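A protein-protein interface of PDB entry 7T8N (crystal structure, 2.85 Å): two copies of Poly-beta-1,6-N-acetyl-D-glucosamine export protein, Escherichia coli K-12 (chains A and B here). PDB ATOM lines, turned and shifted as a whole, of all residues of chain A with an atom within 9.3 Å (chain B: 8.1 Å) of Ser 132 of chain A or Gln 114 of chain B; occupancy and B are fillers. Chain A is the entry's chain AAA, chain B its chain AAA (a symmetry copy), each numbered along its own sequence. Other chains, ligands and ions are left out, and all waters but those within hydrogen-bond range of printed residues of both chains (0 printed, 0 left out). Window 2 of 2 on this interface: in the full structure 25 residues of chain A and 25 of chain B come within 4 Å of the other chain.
No position is printed for both chains.
Of the 11 pairs that touch across the chains among the printed residues, none has its exchanged pair printed and touching as well.
Ser 132 of chain A touches just one residue of chain B: Gln 114 (3.7 Å).
Glu 135 of chain A touches none of the printed residues of chain B.
Tyr 104 of chain B touches none of the printed residues of chain A.
No residue of chain A comes within 4 Å of Ser 115 of chain B.
Of the printed residues of chain A, Met 117 of chain B touches Leu 136 (3.9 Å).
Of the printed residues of chain A, Phe 121 of chain B touches Thr 126.
The nearest residue of chain A that does not touch Gln 114 of chain B is Pro 129 of chain A (5.6 Å).
Hydrophobic or aromatic side chains of chain A that line the printed part of chain B: Leu 136 and Phe 140.
Among the printed residues, no Asp or Glu carboxylate lies within 4 Å of a Lys or Arg side-chain nitrogen of the other chain.
Thr 118 of chain B touches Thr 126 of chain A (CG2 to OG1, 3.9 Å).
Thr 126 of chain A touches Phe 121 of chain B (C to O, 3.8 Å).
C of Ser 132 of chain A touches NE2 of Gln 114 of chain B (3.7 Å).
CD2 of Leu 105 of chain B touches O of Asp 133 of chain A, 3.98 Å away.
Asp 133 of chain A touches Pro 110 of chain B (OD2 to CG, 3.1 Å).
Leu 136 of chain A touches Gln 114 of chain B (CD2 to CD, 3.3 Å).
CD1 of Leu 136 of chain A touches CG of Met 117 of chain B (3.9 Å).
Phe 140 of chain A touches Ala 101 of chain B.
CE2 of Phe 140 of chain A touches CD1 of Leu 105 of chain B (3.2 Å).
The side-chain amide nitrogen (NE2) of Gln 114 of chain B sits at hydrogen-bond distance from the backbone carbonyl oxygen (O) of Leu 131 of chain A (3.2 Å).
The side-chain carboxylate (OD1) of Asp 133 of chain A sits at hydrogen-bond distance from the side-chain amide nitrogen (NE2) of Gln 114 of chain B (3.2 Å).
OG1 of Thr 126 of chain A is in hydrogen-bond range of N of Ala 128 of chain A (3.1 Å).
The side-chain hydroxyl (OG) of Ser 132 of chain A sits close to the side-chain carboxylate (OE1) of Glu 134 of chain A.
The backbone NH (N) of Ser 132 of chain A lies within hydrogen-bond range of the side-chain carboxylate (OE1) of Glu 135 of chain A (3.1 Å).
The backbone carbonyl oxygen (O) of Gln 114 of chain B lies within hydrogen-bond range of the side-chain hydroxyl (OG1) of Thr 118 of chain B (3.0 Å).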
ATOM      1  N   THR A 126      13.822  10.279  -3.293  1.00  0.00           N
ATOM      2  CA  THR A 126      14.608  11.357  -3.945  1.00  0.00           C
ATOM      3  C   THR A 126      13.912  12.718  -3.831  1.00  0.00           C
ATOM      4  O   THR A 126      12.690  12.778  -3.842  1.00  0.00           O
ATOM      5  CB  THR A 126      14.831  11.084  -5.432  1.00  0.00           C
ATOM      6  OG1 THR A 126      15.734  12.093  -5.873  1.00  0.00           O
ATOM      7  CG2 THR A 126      13.547  11.123  -6.234  1.00  0.00           C
ATOM      8  N   ALA A 128      15.251  15.145  -6.115  1.00  0.00           N
ATOM      9  CA  ALA A 128      16.067  15.561  -7.271  1.00  0.00           C
ATOM     10  C   ALA A 128      15.207  16.414  -8.181  1.00  0.00           C
ATOM     11  O   ALA A 128      14.464  15.848  -8.977  1.00  0.00           O
ATOM     12  CB  ALA A 128      16.569  14.340  -8.025  1.00  0.00           C
ATOM     13  N   PRO A 129      15.303  17.761  -8.101  1.00  0.00           N
ATOM     14  CA  PRO A 129      14.784  18.598  -9.168  1.00  0.00           C
ATOM     15  C   PRO A 129      15.231  17.877 -10.443  1.00  0.00           C
ATOM     16  O   PRO A 129      16.406  17.612 -10.587  1.00  0.00           O
ATOM     17  CB  PRO A 129      15.431  19.967  -8.961  1.00  0.00           C
ATOM     18  CG  PRO A 129      15.922  19.964  -7.524  1.00  0.00           C
ATOM     19  CD  PRO A 129      15.939  18.535  -7.033  1.00  0.00           C
ATOM     20  N   ASP A 130      14.292  17.444 -11.273  1.00  0.00           N
ATOM     21  CA  ASP A 130      14.633  16.931 -12.617  1.00  0.00           C
ATOM     22  C   ASP A 130      15.316  18.101 -13.344  1.00  0.00           C
ATOM     23  O   ASP A 130      14.632  19.121 -13.658  1.00  0.00           O
ATOM     24  CB  ASP A 130      13.406  16.329 -13.301  1.00  0.00           C
ATOM     25  CG  ASP A 130      13.735  15.649 -14.615  1.00  0.00           C
ATOM     26  OD1 ASP A 130      14.963  15.424 -14.897  1.00  0.00           O
ATOM     27  OD2 ASP A 130      12.765  15.366 -15.362  1.00  0.00           O
ATOM     28  N   LEU A 131      16.643  18.028 -13.463  1.00  0.00           N
ATOM     29  CA  LEU A 131      17.452  19.040 -14.182  1.00  0.00           C
ATOM     30  C   LEU A 131      17.983  18.367 -15.437  1.00  0.00           C
ATOM     31  O   LEU A 131      18.271  17.160 -15.341  1.00  0.00           O
ATOM     32  CB  LEU A 131      18.584  19.528 -13.275  1.00  0.00           C
ATOM     33  CG  LEU A 131      18.147  20.422 -12.113  1.00  0.00           C
ATOM     34  CD1 LEU A 131      19.327  20.804 -11.233  1.00  0.00           C
ATOM     35  CD2 LEU A 131      17.440  21.676 -12.620  1.00  0.00           C
ATOM     36  N   SER A 132      18.058  19.088 -16.558  1.00  0.00           N
ATOM     37  CA  SER A 132      18.751  18.605 -17.779  1.00  0.00           C
ATOM     38  C   SER A 132      20.266  18.619 -17.524  1.00  0.00           C
ATOM     39  O   SER A 132      20.720  19.309 -16.585  1.00  0.00           O
ATOM     40  CB  SER A 132      18.361  19.397 -18.995  1.00  0.00           C
ATOM     41  OG  SER A 132      18.745  20.756 -18.876  1.00  0.00           O
ATOM     42  N   ASP A 133      21.023  17.852 -18.309  1.00  0.00           N
ATOM     43  CA  ASP A 133      22.506  17.854 -18.277  1.00  0.00           C
ATOM     44  C   ASP A 133      23.006  19.290 -18.490  1.00  0.00           C
ATOM     45  O   ASP A 133      23.953  19.685 -17.792  1.00  0.00           O
ATOM     46  CB  ASP A 133      23.066  16.907 -19.339  1.00  0.00           C
ATOM     47  CG  ASP A 133      22.699  15.436 -19.183  1.00  0.00           C
ATOM     48  OD1 ASP A 133      21.997  15.084 -18.205  1.00  0.00           O
ATOM     49  OD2 ASP A 133      23.130  14.645 -20.046  1.00  0.00           O
ATOM     50  N   GLU A 134      22.376  20.034 -19.413  1.00  0.00           N
ATOM     51  CA  GLU A 134      22.737  21.422 -19.827  1.00  0.00           C
ATOM     52  C   GLU A 134      22.389  22.422 -18.719  1.00  0.00           C
ATOM     53  O   GLU A 134      22.955  23.513 -18.739  1.00  0.00           O
ATOM     54  CB  GLU A 134      22.012  21.830 -21.114  1.00  0.00           C
ATOM     55  CG  GLU A 134      22.275  20.918 -22.304  1.00  0.00           C
ATOM     56  CD  GLU A 134      21.356  19.715 -22.469  1.00  0.00           C
ATOM     57  OE1 GLU A 134      20.374  19.606 -21.724  1.00  0.00           O
ATOM     58  OE2 GLU A 134      21.625  18.886 -23.361  1.00  0.00           O
ATOM     59  N   GLU A 135      21.443  22.067 -17.843  1.00  0.00           N
ATOM     60  CA  GLU A 135      20.966  22.875 -16.684  1.00  0.00           C
ATOM     61  C   GLU A 135      21.824  22.543 -15.470  1.00  0.00           C
ATOM     62  O   GLU A 135      22.150  23.445 -14.701  1.00  0.00           O
ATOM     63  CB  GLU A 135      19.510  22.569 -16.326  1.00  0.00           C
ATOM     64  CG  GLU A 135      18.502  23.266 -17.216  1.00  0.00           C
ATOM     65  CD  GLU A 135      17.065  22.869 -16.939  1.00  0.00           C
ATOM     66  OE1 GLU A 135      16.869  21.889 -16.183  1.00  0.00           O
ATOM     67  OE2 GLU A 135      16.149  23.541 -17.479  1.00  0.00           O
ATOM     68  N   LEU A 136      22.142  21.269 -15.289  1.00  0.00           N
ATOM     69  CA  LEU A 136      23.100  20.851 -14.248  1.00  0.00           C
ATOM     70  C   LEU A 136      24.419  21.538 -14.571  1.00  0.00           C
ATOM     71  O   LEU A 136      25.012  22.089 -13.661  1.00  0.00           O
ATOM     72  CB  LEU A 136      23.220  19.326 -14.247  1.00  0.00           C
ATOM     73  CG  LEU A 136      23.750  18.686 -12.964  1.00  0.00           C
ATOM     74  CD1 LEU A 136      22.968  19.143 -11.742  1.00  0.00           C
ATOM     75  CD2 LEU A 136      23.705  17.174 -13.076  1.00  0.00           C
ATOM     76  N   ALA A 137      24.820  21.550 -15.842  1.00  0.00           N
ATOM     77  CA  ALA A 137      26.056  22.215 -16.313  1.00  0.00           C
ATOM     78  C   ALA A 137      26.020  23.694 -15.909  1.00  0.00           C
ATOM     79  O   ALA A 137      26.945  24.141 -15.218  1.00  0.00           O
ATOM     80  CB  ALA A 137      26.223  22.035 -17.806  1.00  0.00           C
ATOM     81  N   ASP A 138      24.959  24.412 -16.276  1.00  0.00           N
ATOM     82  CA  ASP A 138      24.811  25.865 -16.004  1.00  0.00           C
ATOM     83  C   ASP A 138      24.906  26.116 -14.489  1.00  0.00           C
ATOM     84  O   ASP A 138      24.852  27.277 -14.111  1.00  0.00           O
ATOM     85  CB  ASP A 138      23.525  26.419 -16.640  1.00  0.00           C
ATOM     86  CG  ASP A 138      23.561  26.576 -18.161  1.00  0.00           C
ATOM     87  OD1 ASP A 138      24.461  27.272 -18.670  1.00  0.00           O
ATOM     88  OD2 ASP A 138      22.674  26.020 -18.833  1.00  0.00           O
ATOM     89  N   LEU A 139      25.063  25.082 -13.651  1.00  0.00           N
ATOM     90  CA  LEU A 139      25.194  25.193 -12.164  1.00  0.00           C
ATOM     91  C   LEU A 139      26.675  25.183 -11.735  1.00  0.00           C
ATOM     92  O   LEU A 139      26.933  25.444 -10.542  1.00  0.00           O
ATOM     93  CB  LEU A 139      24.436  24.039 -11.492  1.00  0.00           C
ATOM     94  CG  LEU A 139      23.106  24.388 -10.823  1.00  0.00           C
ATOM     95  CD1 LEU A 139      22.406  23.134 -10.312  1.00  0.00           C
ATOM     96  CD2 LEU A 139      23.303  25.368  -9.682  1.00  0.00           C
ATOM     97  N   PHE A 140      27.605  24.879 -12.654  1.00  0.00           N
ATOM     98  CA  PHE A 140      29.075  24.778 -12.425  1.00  0.00           C
ATOM     99  C   PHE A 140      29.832  25.587 -13.494  1.00  0.00           C
ATOM    100  O   PHE A 140      30.080  26.797 -13.449  1.00  0.00           O
ATOM    101  CB  PHE A 140      29.576  23.327 -12.523  1.00  0.00           C
ATOM    102  CG  PHE A 140      28.892  22.285 -11.658  1.00  0.00           C
ATOM    103  CD1 PHE A 140      28.995  22.302 -10.272  1.00  0.00           C
ATOM    104  CD2 PHE A 140      28.198  21.231 -12.236  1.00  0.00           C
ATOM    105  CE1 PHE A 140      28.372  21.333  -9.496  1.00  0.00           C
ATOM    106  CE2 PHE A 140      27.584  20.261 -11.456  1.00  0.00           C
ATOM    107  CZ  PHE A 140      27.662  20.318 -10.087  1.00  0.00           C
ATOM    108  N   ALA B 101      31.215  16.082  -9.043  1.00  0.00           N
ATOM    109  CA  ALA B 101      30.118  16.216 -10.027  1.00  0.00           C
ATOM    110  C   ALA B 101      30.583  17.188 -11.125  1.00  0.00           C
ATOM    111  O   ALA B 101      30.539  16.808 -12.319  1.00  0.00           O
ATOM    112  CB  ALA B 101      28.844  16.657  -9.364  1.00  0.00           C
ATOM    113  N   TYR B 104      33.005  15.395 -13.352  1.00  0.00           N
ATOM    114  CA  TYR B 104      32.340  14.327 -14.135  1.00  0.00           C
ATOM    115  C   TYR B 104      31.644  14.966 -15.332  1.00  0.00           C
ATOM    116  O   TYR B 104      31.606  14.370 -16.402  1.00  0.00           O
ATOM    117  CB  TYR B 104      31.372  13.546 -13.250  1.00  0.00           C
ATOM    118  CG  TYR B 104      31.935  12.271 -12.684  1.00  0.00           C
ATOM    119  CD1 TYR B 104      32.368  11.248 -13.514  1.00  0.00           C
ATOM    120  CD2 TYR B 104      32.012  12.073 -11.316  1.00  0.00           C
ATOM    121  CE1 TYR B 104      32.869  10.063 -12.994  1.00  0.00           C
ATOM    122  CE2 TYR B 104      32.508  10.894 -10.779  1.00  0.00           C
ATOM    123  CZ  TYR B 104      32.948   9.885 -11.622  1.00  0.00           C
ATOM    124  OH  TYR B 104      33.453   8.718 -11.119  1.00  0.00           O
ATOM    125  N   LEU B 105      31.140  16.174 -15.136  1.00  0.00           N
ATOM    126  CA  LEU B 105      30.378  16.911 -16.172  1.00  0.00           C
ATOM    127  C   LEU B 105      31.327  17.431 -17.241  1.00  0.00           C
ATOM    128  O   LEU B 105      31.021  17.283 -18.431  1.00  0.00           O
ATOM    129  CB  LEU B 105      29.640  18.086 -15.534  1.00  0.00           C
ATOM    130  CG  LEU B 105      28.143  17.874 -15.392  1.00  0.00           C
ATOM    131  CD1 LEU B 105      27.599  18.780 -14.302  1.00  0.00           C
ATOM    132  CD2 LEU B 105      27.437  18.087 -16.726  1.00  0.00           C
ATOM    133  N   GLN B 109      30.588  13.554 -19.209  1.00  0.00           N
ATOM    134  CA  GLN B 109      30.131  12.319 -18.526  1.00  0.00           C
ATOM    135  C   GLN B 109      28.983  12.652 -17.574  1.00  0.00           C
ATOM    136  O   GLN B 109      29.016  12.323 -16.394  1.00  0.00           O
ATOM    137  CB  GLN B 109      31.341  11.691 -17.844  1.00  0.00           C
ATOM    138  CG  GLN B 109      31.160  10.217 -17.560  1.00  0.00           C
ATOM    139  CD  GLN B 109      32.451   9.516 -17.233  1.00  0.00           C
ATOM    140  OE1 GLN B 109      32.535   8.301 -17.354  1.00  0.00           O
ATOM    141  NE2 GLN B 109      33.465  10.266 -16.826  1.00  0.00           N
ATOM    142  N   PRO B 110      27.895  13.267 -18.084  1.00  0.00           N
ATOM    143  CA  PRO B 110      26.908  13.918 -17.228  1.00  0.00           C
ATOM    144  C   PRO B 110      26.050  12.973 -16.373  1.00  0.00           C
ATOM    145  O   PRO B 110      25.703  13.379 -15.309  1.00  0.00           O
ATOM    146  CB  PRO B 110      26.028  14.654 -18.252  1.00  0.00           C
ATOM    147  CG  PRO B 110      26.096  13.782 -19.486  1.00  0.00           C
ATOM    148  CD  PRO B 110      27.538  13.326 -19.508  1.00  0.00           C
ATOM    149  N   LYS B 111      25.723  11.775 -16.873  1.00  0.00           N
ATOM    150  CA  LYS B 111      24.879  10.764 -16.181  1.00  0.00           C
ATOM    151  C   LYS B 111      25.433  10.482 -14.783  1.00  0.00           C
ATOM    152  O   LYS B 111      24.652  10.276 -13.866  1.00  0.00           O
ATOM    153  CB  LYS B 111      24.805   9.463 -16.985  1.00  0.00           C
ATOM    154  CG  LYS B 111      23.991   9.551 -18.267  1.00  0.00           C
ATOM    155  CD  LYS B 111      23.978   8.281 -19.084  1.00  0.00           C
ATOM    156  CE  LYS B 111      23.231   8.454 -20.391  1.00  0.00           C
ATOM    157  NZ  LYS B 111      23.492   7.338 -21.331  1.00  0.00           N
ATOM    158  N   LYS B 112      26.748  10.475 -14.635  1.00  0.00           N
ATOM    159  CA  LYS B 112      27.435  10.232 -13.344  1.00  0.00           C
ATOM    160  C   LYS B 112      27.246  11.463 -12.440  1.00  0.00           C
ATOM    161  O   LYS B 112      27.005  11.281 -11.237  1.00  0.00           O
ATOM    162  CB  LYS B 112      28.892   9.846 -13.622  1.00  0.00           C
ATOM    163  CG  LYS B 112      29.071   8.504 -14.326  1.00  0.00           C
ATOM    164  CD  LYS B 112      30.485   7.953 -14.225  1.00  0.00           C
ATOM    165  CE  LYS B 112      30.683   6.588 -14.862  1.00  0.00           C
ATOM    166  NZ  LYS B 112      32.131   6.283 -15.044  1.00  0.00           N
ATOM    167  N   ALA B 113      27.315  12.675 -12.999  1.00  0.00           N
ATOM    168  CA  ALA B 113      27.104  13.947 -12.269  1.00  0.00           C
ATOM    169  C   ALA B 113      25.688  13.962 -11.678  1.00  0.00           C
ATOM    170  O   ALA B 113      25.527  14.350 -10.497  1.00  0.00           O
ATOM    171  CB  ALA B 113      27.318  15.108 -13.194  1.00  0.00           C
ATOM    172  N   GLN B 114      24.697  13.545 -12.480  1.00  0.00           N
ATOM    173  CA  GLN B 114      23.266  13.483 -12.096  1.00  0.00           C
ATOM    174  C   GLN B 114      23.127  12.541 -10.900  1.00  0.00           C
ATOM    175  O   GLN B 114      22.518  12.975  -9.882  1.00  0.00           O
ATOM    176  CB  GLN B 114      22.396  12.996 -13.257  1.00  0.00           C
ATOM    177  CG  GLN B 114      22.325  13.952 -14.438  1.00  0.00           C
ATOM    178  CD  GLN B 114      21.389  15.110 -14.206  1.00  0.00           C
ATOM    179  OE1 GLN B 114      20.810  15.265 -13.125  1.00  0.00           O
ATOM    180  NE2 GLN B 114      21.246  15.938 -15.232  1.00  0.00           N
ATOM    181  N   SER B 115      23.688  11.327 -11.007  1.00  0.00           N
ATOM    182  CA  SER B 115      23.524  10.255  -9.991  1.00  0.00           C
ATOM    183  C   SER B 115      24.096  10.733  -8.669  1.00  0.00           C
ATOM    184  O   SER B 115      23.504  10.404  -7.637  1.00  0.00           O
ATOM    185  CB  SER B 115      24.104   8.938 -10.394  1.00  0.00           C
ATOM    186  OG  SER B 115      24.968   9.087 -11.491  1.00  0.00           O
ATOM    187  N   ILE B 116      25.166  11.527  -8.721  1.00  0.00           N
ATOM    188  CA  ILE B 116      25.801  12.150  -7.523  1.00  0.00           C
ATOM    189  C   ILE B 116      24.833  13.141  -6.892  1.00  0.00           C
ATOM    190  O   ILE B 116      24.579  13.037  -5.680  1.00  0.00           O
ATOM    191  CB  ILE B 116      27.135  12.818  -7.892  1.00  0.00           C
ATOM    192  CG1 ILE B 116      28.197  11.756  -8.198  1.00  0.00           C
ATOM    193  CG2 ILE B 116      27.603  13.769  -6.796  1.00  0.00           C
ATOM    194  CD1 ILE B 116      29.433  12.293  -8.838  1.00  0.00           C
ATOM    195  N   MET B 117      24.309  14.059  -7.689  1.00  0.00           N
ATOM    196  CA  MET B 117      23.339  15.076  -7.208  1.00  0.00           C
ATOM    197  C   MET B 117      22.090  14.389  -6.648  1.00  0.00           C
ATOM    198  O   MET B 117      21.647  14.771  -5.556  1.00  0.00           O
ATOM    199  CB  MET B 117      22.956  16.028  -8.343  1.00  0.00           C
ATOM    200  CG  MET B 117      24.132  16.850  -8.834  1.00  0.00           C
ATOM    201  SD  MET B 117      25.126  17.505  -7.471  1.00  0.00           S
ATOM    202  CE  MET B 117      24.268  19.038  -7.121  1.00  0.00           C
ATOM    203  N   THR B 118      21.555  13.400  -7.357  1.00  0.00           N
ATOM    204  CA  THR B 118      20.428  12.571  -6.859  1.00  0.00           C
ATOM    205  C   THR B 118      20.793  12.047  -5.463  1.00  0.00           C
ATOM    206  O   THR B 118      20.067  12.349  -4.525  1.00  0.00           O
ATOM    207  CB  THR B 118      20.088  11.442  -7.840  1.00  0.00           C
ATOM    208  OG1 THR B 118      19.754  12.049  -9.087  1.00  0.00           O
ATOM    209  CG2 THR B 118      18.946  10.562  -7.380  1.00  0.00           C
ATOM    210  N   GLU B 119      21.885  11.299  -5.314  1.00  0.00           N
ATOM    211  CA  GLU B 119      22.220  10.639  -4.029  1.00  0.00           C
ATOM    212  C   GLU B 119      22.458  11.675  -2.927  1.00  0.00           C
ATOM    213  O   GLU B 119      22.547  11.280  -1.762  1.00  0.00           O
ATOM    214  CB  GLU B 119      23.458   9.756  -4.175  1.00  0.00           C
ATOM    215  CG  GLU B 119      23.276   8.583  -5.128  1.00  0.00           C
ATOM    216  CD  GLU B 119      21.876   7.990  -5.219  1.00  0.00           C
ATOM    217  OE1 GLU B 119      21.279   7.681  -4.145  1.00  0.00           O
ATOM    218  OE2 GLU B 119      21.375   7.839  -6.371  1.00  0.00           O
ATOM    219  N   LEU B 120      22.604  12.949  -3.285  1.00  0.00           N
ATOM    220  CA  LEU B 120      22.929  14.025  -2.316  1.00  0.00           C
ATOM    221  C   LEU B 120      21.658  14.490  -1.601  1.00  0.00           C
ATOM    222  O   LEU B 120      21.758  14.804  -0.406  1.00  0.00           O
ATOM    223  CB  LEU B 120      23.629  15.171  -3.051  1.00  0.00           C
ATOM    224  CG  LEU B 120      25.156  15.090  -3.051  1.00  0.00           C
ATOM    225  CD1 LEU B 120      25.761  16.112  -4.010  1.00  0.00           C
ATOM    226  CD2 LEU B 120      25.709  15.295  -1.651  1.00  0.00           C
ATOM    227  N   PHE B 121      20.533  14.573  -2.319  1.00  0.00           N
ATOM    228  CA  PHE B 121      19.235  15.141  -1.857  1.00  0.00           C
ATOM    229  C   PHE B 121      18.139  14.073  -1.924  1.00  0.00           C
ATOM    230  O   PHE B 121      17.413  13.946  -2.936  1.00  0.00           O
ATOM    231  CB  PHE B 121      18.843  16.368  -2.693  1.00  0.00           C
ATOM    232  CG  PHE B 121      19.906  17.431  -2.725  1.00  0.00           C
ATOM    233  CD1 PHE B 121      20.067  18.291  -1.654  1.00  0.00           C
ATOM    234  CD2 PHE B 121      20.796  17.504  -3.779  1.00  0.00           C
ATOM    235  CE1 PHE B 121      21.083  19.226  -1.648  1.00  0.00           C
ATOM    236  CE2 PHE B 121      21.812  18.437  -3.774  1.00  0.00           C
ATOM    237  CZ  PHE B 121      21.949  19.301  -2.713  1.00  0.00           C
